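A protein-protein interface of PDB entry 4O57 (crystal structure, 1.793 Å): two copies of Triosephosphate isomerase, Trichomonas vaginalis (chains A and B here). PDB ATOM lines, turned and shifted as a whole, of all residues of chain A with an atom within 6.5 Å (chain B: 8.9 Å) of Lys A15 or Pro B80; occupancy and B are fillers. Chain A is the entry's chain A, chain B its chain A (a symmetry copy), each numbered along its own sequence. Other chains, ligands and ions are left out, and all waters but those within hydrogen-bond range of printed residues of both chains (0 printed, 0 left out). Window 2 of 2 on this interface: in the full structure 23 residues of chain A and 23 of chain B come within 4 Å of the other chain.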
ATOM      1  N   ALA A  12      13.772   6.281  23.691  1.00  0.00           N
ATOM      2  CA  ALA A  12      14.635   6.987  24.666  1.00  0.00           C
ATOM      3  C   ALA A  12      15.650   6.023  25.276  1.00  0.00           C
ATOM      4  O   ALA A  12      15.682   5.823  26.488  1.00  0.00           O
ATOM      5  CB  ALA A  12      13.799   7.673  25.723  1.00  0.00           C
ATOM      6  N   ASN A  13      16.483   5.460  24.416  1.00  0.00           N
ATOM      7  CA  ASN A  13      17.482   4.448  24.782  1.00  0.00           C
ATOM      8  C   ASN A  13      18.682   4.573  23.856  1.00  0.00           C
ATOM      9  O   ASN A  13      18.606   5.177  22.761  1.00  0.00           O
ATOM     10  CB  ASN A  13      16.931   3.019  24.610  1.00  0.00           C
ATOM     11  CG  ASN A  13      15.693   2.737  25.462  1.00  0.00           C
ATOM     12  OD1 ASN A  13      15.812   2.398  26.627  1.00  0.00           O
ATOM     13  ND2 ASN A  13      14.497   2.853  24.872  1.00  0.00           N
ATOM     14  N   PRO A  14      19.818   3.992  24.251  1.00  0.00           N
ATOM     15  CA  PRO A  14      20.142   3.476  25.590  1.00  0.00           C
ATOM     16  C   PRO A  14      20.471   4.596  26.545  1.00  0.00           C
ATOM     17  O   PRO A  14      20.232   5.747  26.228  1.00  0.00           O
ATOM     18  CB  PRO A  14      21.367   2.605  25.328  1.00  0.00           C
ATOM     19  CG  PRO A  14      22.009   3.213  24.161  1.00  0.00           C
ATOM     20  CD  PRO A  14      20.891   3.734  23.292  1.00  0.00           C
ATOM     21  N   LYS A  15      21.033   4.258  27.707  1.00  0.00           N
ATOM     22  CA  LYS A  15      21.107   5.208  28.794  1.00  0.00           C
ATOM     23  C   LYS A  15      22.338   6.076  28.649  1.00  0.00           C
ATOM     24  O   LYS A  15      22.349   7.201  29.110  1.00  0.00           O
ATOM     25  CB  LYS A  15      21.118   4.471  30.137  1.00  0.00           C
ATOM     26  N   THR A  16      23.373   5.554  27.991  1.00  0.00           N
ATOM     27  CA  THR A  16      24.664   6.225  27.950  1.00  0.00           C
ATOM     28  C   THR A  16      25.279   6.170  26.566  1.00  0.00           C
ATOM     29  O   THR A  16      24.936   5.314  25.722  1.00  0.00           O
ATOM     30  CB  THR A  16      25.635   5.574  28.923  1.00  0.00           C
ATOM     31  OG1 THR A  16      26.064   4.313  28.388  1.00  0.00           O
ATOM     32  CG2 THR A  16      24.966   5.369  30.280  1.00  0.00           C
ATOM     33  N   VAL A  17      26.198   7.089  26.319  1.00  0.00           N
ATOM     34  CA  VAL A  17      26.889   7.082  25.038  1.00  0.00           C
ATOM     35  C   VAL A  17      27.724   5.799  24.895  1.00  0.00           C
ATOM     36  O   VAL A  17      27.839   5.256  23.797  1.00  0.00           O
ATOM     37  CB  VAL A  17      27.781   8.346  24.909  1.00  0.00           C
ATOM     38  CG1 VAL A  17      28.766   8.398  26.025  1.00  0.00           C
ATOM     39  CG2 VAL A  17      28.492   8.383  23.570  1.00  0.00           C
ATOM     40  N   GLU A  19      26.973   2.819  26.004  1.00  0.00           N
ATOM     41  CA  GLU A  19      26.082   1.763  25.588  1.00  0.00           C
ATOM     42  C   GLU A  19      25.668   1.967  24.124  1.00  0.00           C
ATOM     43  O   GLU A  19      25.457   1.001  23.404  1.00  0.00           O
ATOM     44  CB  GLU A  19      24.843   1.710  26.463  1.00  0.00           C
ATOM     45  CG  GLU A  19      25.076   1.326  27.909  1.00  0.00           C
ATOM     46  CD  GLU A  19      23.783   1.466  28.672  1.00  0.00           C
ATOM     47  OE1 GLU A  19      22.999   0.496  28.674  1.00  0.00           O
ATOM     48  OE2 GLU A  19      23.513   2.569  29.205  1.00  0.00           O
ATOM     49  N   ALA A  20      25.545   3.215  23.676  1.00  0.00           N
ATOM     50  CA  ALA A  20      25.172   3.429  22.271  1.00  0.00           C
ATOM     51  C   ALA A  20      26.322   2.988  21.375  1.00  0.00           C
ATOM     52  O   ALA A  20      26.101   2.342  20.371  1.00  0.00           O
ATOM     53  CB  ALA A  20      24.792   4.885  21.998  1.00  0.00           C
ATOM     54  N   PHE A  46      22.404  11.402  20.612  1.00  0.00           N
ATOM     55  CA  PHE A  46      23.214  10.316  20.056  1.00  0.00           C
ATOM     56  C   PHE A  46      23.379  10.366  18.541  1.00  0.00           C
ATOM     57  O   PHE A  46      24.164   9.587  17.991  1.00  0.00           O
ATOM     58  CB  PHE A  46      22.609   8.946  20.363  1.00  0.00           C
ATOM     59  CG  PHE A  46      22.634   8.547  21.814  1.00  0.00           C
ATOM     60  CD1 PHE A  46      23.652   8.927  22.667  1.00  0.00           C
ATOM     61  CD2 PHE A  46      21.611   7.768  22.317  1.00  0.00           C
ATOM     62  CE1 PHE A  46      23.648   8.530  24.007  1.00  0.00           C
ATOM     63  CE2 PHE A  46      21.606   7.380  23.637  1.00  0.00           C
ATOM     64  CZ  PHE A  46      22.615   7.761  24.481  1.00  0.00           C
ATOM     65  N   VAL B  65      14.294  18.730  29.690  1.00  0.00           N
ATOM     66  CA  VAL B  65      14.527  17.282  29.809  1.00  0.00           C
ATOM     67  C   VAL B  65      13.232  16.579  30.033  1.00  0.00           C
ATOM     68  O   VAL B  65      12.277  17.198  30.487  1.00  0.00           O
ATOM     69  CB  VAL B  65      15.443  16.941  30.996  1.00  0.00           C
ATOM     70  CG1 VAL B  65      16.807  17.538  30.808  1.00  0.00           C
ATOM     71  CG2 VAL B  65      14.834  17.443  32.268  1.00  0.00           C
ATOM     72  N   PHE B  66      13.175  15.285  29.702  1.00  0.00           N
ATOM     73  CA  PHE B  66      11.953  14.501  29.872  1.00  0.00           C
ATOM     74  C   PHE B  66      11.806  13.957  31.296  1.00  0.00           C
ATOM     75  O   PHE B  66      12.803  13.755  31.989  1.00  0.00           O
ATOM     76  CB  PHE B  66      11.918  13.336  28.875  1.00  0.00           C
ATOM     77  CG  PHE B  66      10.726  12.438  29.045  1.00  0.00           C
ATOM     78  CD1 PHE B  66       9.481  12.818  28.579  1.00  0.00           C
ATOM     79  CD2 PHE B  66      10.855  11.215  29.684  1.00  0.00           C
ATOM     80  CE1 PHE B  66       8.383  11.983  28.741  1.00  0.00           C
ATOM     81  CE2 PHE B  66       9.768  10.383  29.850  1.00  0.00           C
ATOM     82  CZ  PHE B  66       8.530  10.767  29.383  1.00  0.00           C
ATOM     83  N   VAL B  77      14.092  12.934  25.473  1.00  0.00           N
ATOM     84  CA  VAL B  77      15.466  12.845  26.007  1.00  0.00           C
ATOM     85  C   VAL B  77      15.461  12.893  27.549  1.00  0.00           C
ATOM     86  O   VAL B  77      14.671  13.615  28.122  1.00  0.00           O
ATOM     87  CB  VAL B  77      16.304  14.046  25.493  1.00  0.00           C
ATOM     88  CG1 VAL B  77      17.705  14.095  26.143  1.00  0.00           C
ATOM     89  CG2 VAL B  77      16.396  13.995  23.979  1.00  0.00           C
ATOM     90  N   THR B  78      16.368  12.178  28.214  1.00  0.00           N
ATOM     91  CA  THR B  78      16.198  11.903  29.641  1.00  0.00           C
ATOM     92  C   THR B  78      17.402  12.286  30.483  1.00  0.00           C
ATOM     93  O   THR B  78      18.486  12.566  29.977  1.00  0.00           O
ATOM     94  CB  THR B  78      15.901  10.422  29.883  1.00  0.00           C
ATOM     95  OG1 THR B  78      17.118   9.678  29.764  1.00  0.00           O
ATOM     96  CG2 THR B  78      14.872   9.909  28.863  1.00  0.00           C
ATOM     97  N   VAL B  79      17.197  12.296  31.786  1.00  0.00           N
ATOM     98  CA  VAL B  79      18.232  12.787  32.698  1.00  0.00           C
ATOM     99  C   VAL B  79      19.513  11.939  32.677  1.00  0.00           C
ATOM    100  O   VAL B  79      20.611  12.490  32.561  1.00  0.00           O
ATOM    101  CB  VAL B  79      17.706  12.910  34.132  1.00  0.00           C
ATOM    102  CG1 VAL B  79      18.857  13.196  35.103  1.00  0.00           C
ATOM    103  CG2 VAL B  79      16.652  13.993  34.214  1.00  0.00           C
ATOM    104  N   PRO B  80      19.386  10.601  32.792  1.00  0.00           N
ATOM    105  CA  PRO B  80      20.601   9.781  32.708  1.00  0.00           C
ATOM    106  C   PRO B  80      21.435  10.024  31.433  1.00  0.00           C
ATOM    107  O   PRO B  80      22.662  10.043  31.520  1.00  0.00           O
ATOM    108  CB  PRO B  80      20.054   8.355  32.728  1.00  0.00           C
ATOM    109  CG  PRO B  80      18.794   8.447  33.529  1.00  0.00           C
ATOM    110  CD  PRO B  80      18.222   9.821  33.253  1.00  0.00           C
ATOM    111  N   MET B  81      20.798  10.199  30.273  1.00  0.00           N
ATOM    112  CA  MET B  81      21.550  10.435  29.033  1.00  0.00           C
ATOM    113  C   MET B  81      22.385  11.706  29.115  1.00  0.00           C
ATOM    114  O   MET B  81      23.560  11.741  28.704  1.00  0.00           O
ATOM    115  CB  MET B  81      20.612  10.580  27.832  1.00  0.00           C
ATOM    116  CG  MET B  81      19.947   9.309  27.428  1.00  0.00           C
ATOM    117  SD  MET B  81      18.824   9.510  26.017  1.00  0.00           S
ATOM    118  CE  MET B  81      17.660   8.228  26.440  1.00  0.00           C
ATOM    119  N   ILE B  82      21.760  12.779  29.591  1.00  0.00           N
ATOM    120  CA  ILE B  82      22.469  14.032  29.675  1.00  0.00           C
ATOM    121  C   ILE B  82      23.403  13.938  30.869  1.00  0.00           C
ATOM    122  O   ILE B  82      24.569  14.285  30.744  1.00  0.00           O
ATOM    123  CB  ILE B  82      21.528  15.249  29.748  1.00  0.00           C
ATOM    124  CG1 ILE B  82      20.598  15.158  30.954  1.00  0.00           C
ATOM    125  CG2 ILE B  82      20.719  15.344  28.443  1.00  0.00           C
ATOM    126  CD1 ILE B  82      19.815  16.415  31.177  1.00  0.00           C
ATOM    127  N   LYS B  83      22.901  13.411  31.991  1.00  0.00           N
ATOM    128  CA  LYS B  83      23.715  13.182  33.204  1.00  0.00           C
ATOM    129  C   LYS B  83      24.928  12.335  32.858  1.00  0.00           C
ATOM    130  O   LYS B  83      26.030  12.626  33.296  1.00  0.00           O
ATOM    131  N   SER B  84      24.718  11.300  32.046  1.00  0.00           N
ATOM    132  CA  SER B  84      25.779  10.368  31.681  1.00  0.00           C
ATOM    133  C   SER B  84      26.773  11.026  30.732  1.00  0.00           C
ATOM    134  O   SER B  84      27.935  10.619  30.676  1.00  0.00           O
ATOM    135  N   PHE B  85      26.316  12.045  29.996  1.00  0.00           N
ATOM    136  CA  PHE B  85      27.201  12.848  29.142  1.00  0.00           C
ATOM    137  C   PHE B  85      28.040  13.866  29.937  1.00  0.00           C
ATOM    138  O   PHE B  85      28.979  14.473  29.407  1.00  0.00           O
ATOM    139  N   GLY B  86      27.704  14.055  31.212  1.00  0.00           N
ATOM    140  CA  GLY B  86      28.383  15.045  32.032  1.00  0.00           C
ATOM    141  C   GLY B  86      27.717  16.412  31.963  1.00  0.00           C
ATOM    142  O   GLY B  86      28.333  17.435  32.263  1.00  0.00           O
ATOM    143  N   ILE B  87      26.454  16.439  31.563  1.00  0.00           N
ATOM    144  CA  ILE B  87      25.716  17.708  31.506  1.00  0.00           C
ATOM    145  C   ILE B  87      24.986  17.878  32.819  1.00  0.00           C
ATOM    146  O   ILE B  87      24.272  16.971  33.261  1.00  0.00           O
ATOM    147  CB  ILE B  87      24.785  17.746  30.297  1.00  0.00           C
ATOM    148  CG1 ILE B  87      25.658  17.903  29.059  1.00  0.00           C
ATOM    149  CG2 ILE B  87      23.774  18.897  30.404  1.00  0.00           C
ATOM    150  CD1 ILE B  87      24.983  17.592  27.806  1.00  0.00           C
ATOM    151  N   PHE B 114      12.229  15.817  40.391  1.00  0.00           N
ATOM    152  CA  PHE B 114      12.886  14.691  39.773  1.00  0.00           C
ATOM    153  C   PHE B 114      14.297  15.008  39.277  1.00  0.00           C
ATOM    154  O   PHE B 114      15.211  14.186  39.440  1.00  0.00           O
ATOM    155  CB  PHE B 114      12.041  14.140  38.630  1.00  0.00           C
ATOM    156  CG  PHE B 114      12.655  12.948  37.957  1.00  0.00           C
ATOM    157  CD1 PHE B 114      12.435  11.665  38.445  1.00  0.00           C
ATOM    158  CD2 PHE B 114      13.486  13.109  36.853  1.00  0.00           C
ATOM    159  CE1 PHE B 114      13.010  10.570  37.833  1.00  0.00           C
ATOM    160  CE2 PHE B 114      14.050  12.000  36.224  1.00  0.00           C
ATOM    161  CZ  PHE B 114      13.826  10.743  36.722  1.00  0.00           C
ATOM    162  N   ALA B 115      14.471  16.154  38.618  1.00  0.00           N
ATOM    163  CA  ALA B 115      15.790  16.547  38.138  1.00  0.00           C
ATOM    164  C   ALA B 115      16.793  16.697  39.292  1.00  0.00           C
ATOM    165  O   ALA B 115      17.938  16.256  39.188  1.00  0.00           O
ATOM    166  CB  ALA B 115      15.716  17.875  37.351  1.00  0.00           C
ATOM    167  N   ASN B 118      18.021  13.609  40.932  1.00  0.00           N
ATOM    168  CA  ASN B 118      19.000  12.935  40.075  1.00  0.00           C
ATOM    169  C   ASN B 118      20.298  13.698  39.822  1.00  0.00           C
ATOM    170  O   ASN B 118      21.048  13.375  38.903  1.00  0.00           O
ATOM    171  CB  ASN B 118      18.363  12.577  38.739  1.00  0.00           C
ATOM    172  CG  ASN B 118      17.491  11.377  38.840  1.00  0.00           C
ATOM    173  OD1 ASN B 118      17.962  10.252  38.671  1.00  0.00           O
ATOM    174  ND2 ASN B 118      16.220  11.587  39.153  1.00  0.00           N
ATOM    175  N   MET B 120      20.886  16.867  39.016  1.00  0.00           N
ATOM    176  CA  MET B 120      20.833  18.013  38.077  1.00  0.00           C
ATOM    177  C   MET B 120      20.656  19.345  38.783  1.00  0.00           C
ATOM    178  O   MET B 120      19.942  19.416  39.796  1.00  0.00           O
ATOM    179  CB  MET B 120      19.646  17.884  37.111  1.00  0.00           C
ATOM    180  CG  MET B 120      19.646  16.653  36.219  1.00  0.00           C
ATOM    181  SD  MET B 120      21.029  16.574  35.075  1.00  0.00           S
ATOM    182  CE  MET B 120      20.697  17.985  34.021  1.00  0.00           C
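Of the 9 printed residues of chain A, 4 touch a printed residue of chain B. Hydrophobic or aromatic side chains of chain B that line the printed part of chain A: Met B81.
Lys A15 touches two residues of chain B. Pro B80 touches just one residue of chain A: Lys A15 (3.7 Å). Pro A14 touches one residue of chain B. No residue of chain B comes within 4 Å of Thr A16. Printed residues of chain B within 4 Å of Ala A12: Met B81. Of the printed residues of chain B, Asn A13 touches Met B81. Of the printed residues of chain A, Met B81 touches Ala A12, Asn A13, Pro A14 and Lys A15. Ile B87 touches none of the printed residues of chain A.
No position is printed for both chains.
N of Lys A15 sits close to OE2 of Glu A19.
Met B81 touches Ala A12 (CE to O, 3.1 Å). CE of Met B81 touches N of Asn A13, at 3.6 Å. Pro A14 touches Met B81 (O to CE, 3.6 Å). O of Lys A15 touches O of Pro B80 (3.7 Å). O of Lys A15 touches CA of Met B81, at 3.3 Å.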
